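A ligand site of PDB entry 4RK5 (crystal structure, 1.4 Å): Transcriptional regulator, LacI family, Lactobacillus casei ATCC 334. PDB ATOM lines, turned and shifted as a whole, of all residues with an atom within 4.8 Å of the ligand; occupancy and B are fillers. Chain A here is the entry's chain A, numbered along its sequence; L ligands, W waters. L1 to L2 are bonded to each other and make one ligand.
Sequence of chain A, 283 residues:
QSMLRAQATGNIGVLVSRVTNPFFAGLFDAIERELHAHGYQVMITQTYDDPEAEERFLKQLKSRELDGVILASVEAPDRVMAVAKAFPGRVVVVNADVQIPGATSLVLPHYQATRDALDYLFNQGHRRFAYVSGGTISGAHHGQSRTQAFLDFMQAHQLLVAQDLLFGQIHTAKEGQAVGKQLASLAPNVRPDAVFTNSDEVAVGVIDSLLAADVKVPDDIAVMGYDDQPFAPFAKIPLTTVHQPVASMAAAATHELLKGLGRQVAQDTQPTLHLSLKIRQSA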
ATOM      1  N   SER A  17      -6.029 -26.078   9.249  1.00  0.00           N
ATOM      2  CA  SER A  17      -5.184 -24.956   9.618  1.00  0.00           C
ATOM      3  C   SER A  17      -5.919 -23.633   9.918  1.00  0.00           C
ATOM      4  O   SER A  17      -5.507 -22.903  10.772  1.00  0.00           O
ATOM      5  CB  SER A  17      -3.989 -24.803   8.687  1.00  0.00           C
ATOM      6  OG  SER A  17      -4.408 -24.405   7.424  1.00  0.00           O
ATOM      7  N   ARG A  18      -6.987 -23.324   9.178  1.00  0.00           N
ATOM      8  CA  ARG A  18      -7.646 -22.000   9.300  1.00  0.00           C
ATOM      9  C   ARG A  18      -9.079 -22.083   8.800  1.00  0.00           C
ATOM     10  O   ARG A  18      -9.291 -22.396   7.634  1.00  0.00           O
ATOM     11  CB  ARG A  18      -6.840 -20.948   8.552  1.00  0.00           C
ATOM     12  CG  ARG A  18      -7.440 -19.566   8.595  1.00  0.00           C
ATOM     13  CD  ARG A  18      -6.498 -18.489   8.024  1.00  0.00           C
ATOM     14  NE  ARG A  18      -6.083 -18.769   6.699  1.00  0.00           N
ATOM     15  CZ  ARG A  18      -6.730 -18.388   5.592  1.00  0.00           C
ATOM     16  NH1 ARG A  18      -7.822 -17.633   5.619  1.00  0.00           N
ATOM     17  NH2 ARG A  18      -6.225 -18.737   4.415  1.00  0.00           N
ATOM     18  N   ASN A  21     -10.354 -19.891   5.818  1.00  0.00           N
ATOM     19  CA  ASN A  21     -10.074 -20.337   4.457  1.00  0.00           C
ATOM     20  C   ASN A  21     -11.366 -20.982   3.947  1.00  0.00           C
ATOM     21  O   ASN A  21     -11.782 -22.029   4.477  1.00  0.00           O
ATOM     22  CB  ASN A  21      -8.937 -21.343   4.481  1.00  0.00           C
ATOM     23  CG  ASN A  21      -8.617 -21.893   3.133  1.00  0.00           C
ATOM     24  OD1 ASN A  21      -9.442 -21.867   2.219  1.00  0.00           O
ATOM     25  ND2 ASN A  21      -7.451 -22.490   3.027  1.00  0.00           N
ATOM     26  N   PHE A  23     -12.098 -22.853   1.560  1.00  0.00           N
ATOM     27  CA  PHE A  23     -11.932 -24.250   1.228  1.00  0.00           C
ATOM     28  C   PHE A  23     -12.183 -25.123   2.475  1.00  0.00           C
ATOM     29  O   PHE A  23     -12.929 -26.119   2.430  1.00  0.00           O
ATOM     30  CB  PHE A  23     -10.549 -24.530   0.650  1.00  0.00           C
ATOM     31  CG  PHE A  23     -10.257 -26.001   0.538  1.00  0.00           C
ATOM     32  CD1 PHE A  23     -10.805 -26.744  -0.512  1.00  0.00           C
ATOM     33  CD2 PHE A  23      -9.502 -26.638   1.471  1.00  0.00           C
ATOM     34  CE1 PHE A  23     -10.632 -28.077  -0.537  1.00  0.00           C
ATOM     35  CE2 PHE A  23      -9.334 -28.008   1.417  1.00  0.00           C
ATOM     36  CZ  PHE A  23      -9.909 -28.721   0.396  1.00  0.00           C
ATOM     37  N   PHE A  24     -11.548 -24.757   3.587  1.00  0.00           N
ATOM     38  CA  PHE A  24     -11.728 -25.555   4.794  1.00  0.00           C
ATOM     39  C   PHE A  24     -13.140 -25.394   5.364  1.00  0.00           C
ATOM     40  O   PHE A  24     -13.691 -26.389   5.855  1.00  0.00           O
ATOM     41  CB  PHE A  24     -10.677 -25.185   5.841  1.00  0.00           C
ATOM     42  CG  PHE A  24      -9.305 -25.756   5.627  1.00  0.00           C
ATOM     43  CD1 PHE A  24      -9.120 -27.097   5.321  1.00  0.00           C
ATOM     44  CD2 PHE A  24      -8.176 -24.961   5.741  1.00  0.00           C
ATOM     45  CE1 PHE A  24      -7.863 -27.631   5.199  1.00  0.00           C
ATOM     46  CE2 PHE A  24      -6.904 -25.520   5.587  1.00  0.00           C
ATOM     47  CZ  PHE A  24      -6.777 -26.861   5.339  1.00  0.00           C
ATOM     48  N   ASP A  49      -1.100 -23.919  11.810  1.00  0.00           N
ATOM     49  CA  ASP A  49       0.186 -24.662  11.564  1.00  0.00           C
ATOM     50  C   ASP A  49       1.034 -24.914  12.812  1.00  0.00           C
ATOM     51  O   ASP A  49       2.206 -25.255  12.702  1.00  0.00           O
ATOM     52  CB  ASP A  49       1.060 -23.920  10.568  1.00  0.00           C
ATOM     53  CG  ASP A  49       0.414 -23.839   9.218  1.00  0.00           C
ATOM     54  OD1 ASP A  49      -0.334 -24.783   8.876  1.00  0.00           O
ATOM     55  OD2 ASP A  49       0.594 -22.805   8.538  1.00  0.00           O
ATOM     56  N   ALA A  72      -7.689 -32.522   7.944  1.00  0.00           N
ATOM     57  CA  ALA A  72      -7.519 -32.046   6.592  1.00  0.00           C
ATOM     58  C   ALA A  72      -6.217 -31.260   6.415  1.00  0.00           C
ATOM     59  O   ALA A  72      -5.924 -30.723   5.318  1.00  0.00           O
ATOM     60  CB  ALA A  72      -8.712 -31.207   6.124  1.00  0.00           C
ATOM     61  N   SER A  73      -5.418 -31.191   7.486  1.00  0.00           N
ATOM     62  CA  SER A  73      -4.073 -30.708   7.476  1.00  0.00           C
ATOM     63  C   SER A  73      -3.325 -31.467   8.543  1.00  0.00           C
ATOM     64  O   SER A  73      -3.908 -31.887   9.508  1.00  0.00           O
ATOM     65  CB  SER A  73      -4.052 -29.213   7.646  1.00  0.00           C
ATOM     66  OG  SER A  73      -4.724 -28.794   8.748  1.00  0.00           O
ATOM     67  N   GLU A  75       0.530 -31.471  10.686  1.00  0.00           N
ATOM     68  CA  GLU A  75       1.770 -30.781  11.042  1.00  0.00           C
ATOM     69  C   GLU A  75       2.909 -31.726  11.361  1.00  0.00           C
ATOM     70  O   GLU A  75       4.041 -31.530  10.895  1.00  0.00           O
ATOM     71  CB  GLU A  75       1.511 -29.861  12.231  1.00  0.00           C
ATOM     72  CG  GLU A  75       0.471 -28.839  11.921  1.00  0.00           C
ATOM     73  CD  GLU A  75       0.683 -28.088  10.568  1.00  0.00           C
ATOM     74  OE1 GLU A  75       1.859 -27.780  10.239  1.00  0.00           O
ATOM     75  OE2 GLU A  75      -0.372 -27.840   9.852  1.00  0.00           O
ATOM     76  N   ASN A  95      -6.692 -35.141   2.085  1.00  0.00           N
ATOM     77  CA  ASN A  95      -6.169 -34.049   1.266  1.00  0.00           C
ATOM     78  C   ASN A  95      -5.030 -33.264   1.918  1.00  0.00           C
ATOM     79  O   ASN A  95      -4.897 -32.074   1.684  1.00  0.00           O
ATOM     80  CB  ASN A  95      -7.313 -33.116   0.849  1.00  0.00           C
ATOM     81  CG  ASN A  95      -6.953 -32.265  -0.341  1.00  0.00           C
ATOM     82  OD1 ASN A  95      -6.250 -32.718  -1.251  1.00  0.00           O
ATOM     83  ND2 ASN A  95      -7.448 -31.040  -0.350  1.00  0.00           N
ATOM     84  N   HIS A 110      -2.274 -33.254  -6.513  1.00  0.00           N
ATOM     85  CA  HIS A 110      -1.937 -31.862  -6.655  1.00  0.00           C
ATOM     86  C   HIS A 110      -0.720 -31.573  -7.523  1.00  0.00           C
ATOM     87  O   HIS A 110      -0.672 -30.555  -8.179  1.00  0.00           O
ATOM     88  CB  HIS A 110      -1.819 -31.195  -5.304  1.00  0.00           C
ATOM     89  CG  HIS A 110      -3.122 -31.137  -4.586  1.00  0.00           C
ATOM     90  ND1 HIS A 110      -4.104 -30.221  -4.899  1.00  0.00           N
ATOM     91  CD2 HIS A 110      -3.602 -31.880  -3.556  1.00  0.00           C
ATOM     92  CE1 HIS A 110      -5.135 -30.416  -4.089  1.00  0.00           C
ATOM     93  NE2 HIS A 110      -4.858 -31.418  -3.268  1.00  0.00           N
ATOM     94  N   GLY A 134       1.770 -20.715   0.345  1.00  0.00           N
ATOM     95  CA  GLY A 134       1.498 -20.517   1.727  1.00  0.00           C
ATOM     96  C   GLY A 134       2.621 -20.961   2.647  1.00  0.00           C
ATOM     97  O   GLY A 134       2.574 -20.644   3.827  1.00  0.00           O
ATOM     98  N   GLY A 135       3.588 -21.656   2.123  1.00  0.00           N
ATOM     99  CA  GLY A 135       4.743 -22.090   2.875  1.00  0.00           C
ATOM    100  C   GLY A 135       5.975 -21.283   2.566  1.00  0.00           C
ATOM    101  O   GLY A 135       5.956 -20.310   1.800  1.00  0.00           O
ATOM    102  N   HIS A 142       4.042 -27.138   3.785  1.00  0.00           N
ATOM    103  CA  HIS A 142       2.780 -27.501   3.166  1.00  0.00           C
ATOM    104  C   HIS A 142       2.627 -26.973   1.768  1.00  0.00           C
ATOM    105  O   HIS A 142       3.007 -25.826   1.415  1.00  0.00           O
ATOM    106  CB  HIS A 142       1.595 -27.060   3.974  1.00  0.00           C
ATOM    107  CG  HIS A 142       1.612 -27.605   5.343  1.00  0.00           C
ATOM    108  ND1 HIS A 142       2.753 -28.087   5.946  1.00  0.00           N
ATOM    109  CD2 HIS A 142       0.623 -27.712   6.264  1.00  0.00           C
ATOM    110  CE1 HIS A 142       2.443 -28.500   7.165  1.00  0.00           C
ATOM    111  NE2 HIS A 142       1.176 -28.261   7.389  1.00  0.00           N
ATOM    112  N   GLY A 143       2.069 -27.843   0.965  1.00  0.00           N
ATOM    113  CA  GLY A 143       1.895 -27.544  -0.491  1.00  0.00           C
ATOM    114  C   GLY A 143       3.193 -27.751  -1.269  1.00  0.00           C
ATOM    115  O   GLY A 143       3.396 -27.207  -2.325  1.00  0.00           O
ATOM    116  N   ARG A 146       3.108 -29.112  -4.892  1.00  0.00           N
ATOM    117  CA  ARG A 146       2.852 -28.026  -5.829  1.00  0.00           C
ATOM    118  C   ARG A 146       4.135 -27.235  -6.189  1.00  0.00           C
ATOM    119  O   ARG A 146       4.376 -26.897  -7.336  1.00  0.00           O
ATOM    120  CB  ARG A 146       1.769 -27.097  -5.336  1.00  0.00           C
ATOM    121  CG  ARG A 146       0.495 -27.814  -5.013  1.00  0.00           C
ATOM    122  CD  ARG A 146      -0.456 -26.881  -4.462  1.00  0.00           C
ATOM    123  NE  ARG A 146      -1.556 -27.544  -3.850  1.00  0.00           N
ATOM    124  CZ  ARG A 146      -2.617 -26.889  -3.337  1.00  0.00           C
ATOM    125  NH1 ARG A 146      -2.717 -25.556  -3.472  1.00  0.00           N
ATOM    126  NH2 ARG A 146      -3.576 -27.530  -2.746  1.00  0.00           N
ATOM    127  N   HIS A 171      -1.201 -16.200   2.410  1.00  0.00           N
ATOM    128  CA  HIS A 171      -2.408 -16.992   2.665  1.00  0.00           C
ATOM    129  C   HIS A 171      -3.707 -16.285   2.354  1.00  0.00           C
ATOM    130  O   HIS A 171      -4.666 -16.906   1.845  1.00  0.00           O
ATOM    131  CB  HIS A 171      -2.456 -17.404   4.145  1.00  0.00           C
ATOM    132  CG  HIS A 171      -1.288 -18.153   4.612  1.00  0.00           C
ATOM    133  ND1 HIS A 171      -0.350 -17.634   5.455  1.00  0.00           N
ATOM    134  CD2 HIS A 171      -0.847 -19.375   4.281  1.00  0.00           C
ATOM    135  CE1 HIS A 171       0.617 -18.532   5.620  1.00  0.00           C
ATOM    136  NE2 HIS A 171       0.326 -19.589   4.920  1.00  0.00           N
ATOM    137  N   ASN A 198      -1.736 -20.290  -5.750  1.00  0.00           N
ATOM    138  CA  ASN A 198      -1.974 -21.365  -4.788  1.00  0.00           C
ATOM    139  C   ASN A 198      -3.221 -21.178  -3.926  1.00  0.00           C
ATOM    140  O   ASN A 198      -3.441 -21.979  -2.994  1.00  0.00           O
ATOM    141  CB  ASN A 198      -0.731 -21.649  -3.943  1.00  0.00           C
ATOM    142  CG  ASN A 198       0.030 -22.838  -4.413  1.00  0.00           C
ATOM    143  OD1 ASN A 198      -0.547 -23.906  -4.646  1.00  0.00           O
ATOM    144  ND2 ASN A 198       1.331 -22.694  -4.580  1.00  0.00           N
ATOM    145  N   SER A 199      -4.068 -20.198  -4.244  1.00  0.00           N
ATOM    146  CA  SER A 199      -5.219 -19.969  -3.380  1.00  0.00           C
ATOM    147  C   SER A 199      -6.113 -18.902  -4.021  1.00  0.00           C
ATOM    148  O   SER A 199      -5.686 -17.808  -4.391  1.00  0.00           O
ATOM    149  CB  SER A 199      -4.762 -19.364  -2.042  1.00  0.00           C
ATOM    150  OG  SER A 199      -5.801 -18.655  -1.409  1.00  0.00           O
ATOM    151  N   TYR A 226      -6.457 -21.161  -6.919  1.00  0.00           N
ATOM    152  CA  TYR A 226      -6.480 -22.579  -6.580  1.00  0.00           C
ATOM    153  C   TYR A 226      -7.618 -22.815  -5.618  1.00  0.00           C
ATOM    154  O   TYR A 226      -7.763 -22.077  -4.630  1.00  0.00           O
ATOM    155  CB  TYR A 226      -5.163 -23.045  -5.927  1.00  0.00           C
ATOM    156  CG  TYR A 226      -4.775 -24.492  -6.208  1.00  0.00           C
ATOM    157  CD1 TYR A 226      -5.439 -25.553  -5.601  1.00  0.00           C
ATOM    158  CD2 TYR A 226      -3.758 -24.818  -7.052  1.00  0.00           C
ATOM    159  CE1 TYR A 226      -5.077 -26.855  -5.863  1.00  0.00           C
ATOM    160  CE2 TYR A 226      -3.326 -26.094  -7.279  1.00  0.00           C
ATOM    161  CZ  TYR A 226      -4.017 -27.135  -6.697  1.00  0.00           C
ATOM    162  OH  TYR A 226      -3.610 -28.424  -6.934  1.00  0.00           O
ATOM    163  N   ASP A 227      -8.431 -23.818  -5.925  1.00  0.00           N
ATOM    164  CA  ASP A 227      -9.469 -24.464  -5.082  1.00  0.00           C
ATOM    165  C   ASP A 227     -10.854 -24.435  -5.749  1.00  0.00           C
ATOM    166  O   ASP A 227     -11.597 -25.413  -5.601  1.00  0.00           O
ATOM    167  CB  ASP A 227      -9.650 -23.895  -3.683  1.00  0.00           C
ATOM    168  CG  ASP A 227      -8.455 -24.105  -2.754  1.00  0.00           C
ATOM    169  OD1 ASP A 227      -7.564 -24.906  -3.076  1.00  0.00           O
ATOM    170  OD2 ASP A 227      -8.511 -23.434  -1.712  1.00  0.00           O
ATOM    171  N   GLN A 229     -13.147 -21.947  -4.863  1.00  0.00           N
ATOM    172  CA  GLN A 229     -13.909 -21.579  -3.700  1.00  0.00           C
ATOM    173  C   GLN A 229     -15.251 -20.940  -4.088  1.00  0.00           C
ATOM    174  O   GLN A 229     -15.430 -20.504  -5.215  1.00  0.00           O
ATOM    175  CB  GLN A 229     -13.098 -20.629  -2.793  1.00  0.00           C
ATOM    176  CG  GLN A 229     -11.882 -21.332  -2.231  1.00  0.00           C
ATOM    177  CD  GLN A 229     -10.953 -20.427  -1.447  1.00  0.00           C
ATOM    178  OE1 GLN A 229     -11.291 -19.285  -1.113  1.00  0.00           O
ATOM    179  NE2 GLN A 229      -9.769 -20.945  -1.134  1.00  0.00           N
ATOM    180  N   GLN A 244     -11.078 -28.137  -6.686  1.00  0.00           N
ATOM    181  CA  GLN A 244     -11.017 -29.274  -5.759  1.00  0.00           C
ATOM    182  C   GLN A 244     -12.426 -29.822  -5.547  1.00  0.00           C
ATOM    183  O   GLN A 244     -13.360 -29.054  -5.316  1.00  0.00           O
ATOM    184  CB  GLN A 244     -10.401 -28.879  -4.415  1.00  0.00           C
ATOM    185  CG  GLN A 244      -8.943 -28.444  -4.529  1.00  0.00           C
ATOM    186  CD  GLN A 244      -8.150 -28.726  -3.281  1.00  0.00           C
ATOM    187  OE1 GLN A 244      -8.088 -29.893  -2.864  1.00  0.00           O
ATOM    188  NE2 GLN A 244      -7.544 -27.719  -2.714  1.00  0.00           N
HETATM  189  C1  LIG L   1      -4.970 -25.580   2.422  1.00  0.00           C
HETATM  190  C2  LIG L   1      -5.507 -26.819   1.716  1.00  0.00           C
HETATM  191  C3  LIG L   1      -5.138 -26.847   0.244  1.00  0.00           C
HETATM  192  C4  LIG L   1      -5.691 -25.568  -0.371  1.00  0.00           C
HETATM  193  C5  LIG L   1      -5.028 -24.386   0.338  1.00  0.00           C
HETATM  194  C6  LIG L   1      -5.460 -23.010  -0.132  1.00  0.00           C
HETATM  195  O1  LIG L   1      -4.998 -27.998   2.400  1.00  0.00           O
HETATM  196  O2  LIG L   1      -5.751 -27.981  -0.379  1.00  0.00           O
HETATM  197  O3  LIG L   1      -5.364 -25.507  -1.764  1.00  0.00           O
HETATM  198  O4  LIG L   1      -5.363 -24.406   1.758  1.00  0.00           O
HETATM  199  O5  LIG L   1      -6.860 -22.777   0.139  1.00  0.00           O
HETATM  200  C1  LG2 L   2      -2.846 -26.524   4.639  1.00  0.00           C
HETATM  201  C2  LG2 L   2      -2.921 -25.315   3.711  1.00  0.00           C
HETATM  202  C3  LG2 L   2      -1.597 -24.650   3.360  1.00  0.00           C
HETATM  203  C4  LG2 L   2      -2.051 -23.245   3.005  1.00  0.00           C
HETATM  204  C5  LG2 L   2      -3.057 -22.988   4.113  1.00  0.00           C
HETATM  205  C6  LG2 L   2      -4.131 -21.996   3.778  1.00  0.00           C
HETATM  206  O1  LG2 L   2      -2.342 -26.156   5.937  1.00  0.00           O
HETATM  207  O2  LG2 L   2      -3.527 -25.684   2.459  1.00  0.00           O
HETATM  208  O3  LG2 L   2      -0.900 -25.355   2.318  1.00  0.00           O
HETATM  209  O4  LG2 L   2      -0.991 -22.302   3.022  1.00  0.00           O
HETATM  210  O5  LG2 L   2      -3.661 -24.292   4.366  1.00  0.00           O
HETATM  211  O6  LG2 L   2      -5.087 -21.789   4.796  1.00  0.00           O
HETATM  212  O   HOH W   1      -3.966 -30.097  -0.148  1.00  0.00           O
HETATM  213  O   HOH W   2      -7.116 -20.111   0.370  1.00  0.00           O
HETATM  214  O   HOH W   3      -6.671 -30.160   2.723  1.00  0.00           O
HETATM  215  O   HOH W   4      -3.354 -30.020   4.198  1.00  0.00           O
HETATM  216  O   HOH W   5       0.200 -23.202   6.013  1.00  0.00           O
HETATM  217  O   HOH W   6      -4.478 -19.562   1.555  1.00  0.00           O
HETATM  218  O   HOH W   7      -1.564 -25.879  -0.229  1.00  0.00           O
HETATM  219  O   HOH W   8      -2.165 -20.778   0.557  1.00  0.00           O
HETATM  220  O   HOH W   9      -2.298 -28.755   1.684  1.00  0.00           O
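The side-chain carboxylate (OD2) of Asp 227 is in hydrogen-bond range of an oxygen (O5) of LIG L1. The guanidinium group (NH2) of Arg 146 is in hydrogen-bond range of an oxygen (O3) of LIG L1 (2.9 Å). The side-chain amide nitrogen of Gln 244 is in hydrogen-bond range of an oxygen (O2) of LIG L1 (3.0 Å). O5 of LIG L1 is in hydrogen-bond range of ND2 of Asn 21 (3.0 Å). OG of Ser 17 lies within hydrogen-bond range of O1 of LG2 L2. NH2 of Arg 18 sits at hydrogen-bond distance from O6 of LG2 L2 (3.3 Å). The side-chain amide nitrogen (ND2) of Asn 95 sits at hydrogen-bond distance from an oxygen (O2) of LIG L1.
The side-chain carboxylate of Asp 227 sits at hydrogen-bond distance from the side-chain amide nitrogen of Gln 244. NE2 of Gln 229 lies within hydrogen-bond range of OD2 of Asp 227 (2.8 Å). The guanidinium group (NH1) of Arg 146 is in hydrogen-bond range of the side-chain amide oxygen (OD1) of Asn 198 (3.0 Å). NH2 of Arg 146 is in hydrogen-bond range of ND1 of His 110 (3.5 Å). The side-chain amide nitrogen (NE2) of Gln 229 is in hydrogen-bond range of the side-chain amide oxygen (OD1) of Asn 21 (3.5 Å). The backbone NH of Ser 17 sits at hydrogen-bond distance from the side-chain hydroxyl of Ser 73 (3.1 Å). NE2 of His 171 lies within hydrogen-bond range of O of Gly 134 (2.7 Å). OD1 of Asn 95 lies within hydrogen-bond range of NE2 of His 110.
CZ of Phe 24 touches O1 of LIG L1, at 3.6 Å. Asp 49 touches the ligand. Ser 73 touches the ligand. CA of Gly 134 touches O4 of LG2 L2, at 3.3 Å. CD2 of His 142 touches O1 of LG2 L2, 3.4 Å away. CD2 of His 171 touches O4 of LG2 L2 (3.2 Å). O of Asn 198 touches C6 of LIG L1 (3.7 Å). CD1 of Tyr 226 touches O3 of LIG L1, 3.8 Å away. NE2 of Gln 229 touches O5 of LIG L1, at 3.7 Å. Within 4 Å of the ligand: Ser 17, Arg 18, Asn 21, Phe 24, Asp 49, Ser 73, Asn 95, Gly 134, His 142, Arg 146, His 171, Asn 198, Tyr 226, Asp 227, Gln 229 and Gln 244.
Water W7 bridges an oxygen (O3) of LG2 L2 (2.7 Å) and the guanidinium group of Arg 146 (3.5 Å). Water W2 lies within hydrogen-bond range of the side-chain hydroxyl of Ser 199 (2.6 Å), an oxygen (O5) of LIG L1 (2.7 Å), the side-chain amide nitrogen of Gln 229 (3.2 Å) and the side-chain amide oxygen of Asn 21 (3.5 Å). Water W1 lies within hydrogen-bond range of an oxygen (O2) of LIG L1 and the backbone carbonyl oxygen (O) of Asn 95. Water W4 bridges the backbone carbonyl oxygen (O) of Ala 72 and an oxygen (O1) of LIG L1. Water W6 lies within hydrogen-bond range of the backbone carbonyl oxygen (O) of His 171 (2.7 Å), the side-chain hydroxyl (OG) of Ser 199 (3.4 Å) and the guanidinium group (NH2) of Arg 18 (3.5 Å). Water W5 bridges the side-chain carboxylate of Asp 49 and an oxygen (O4) of LG2 L2.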
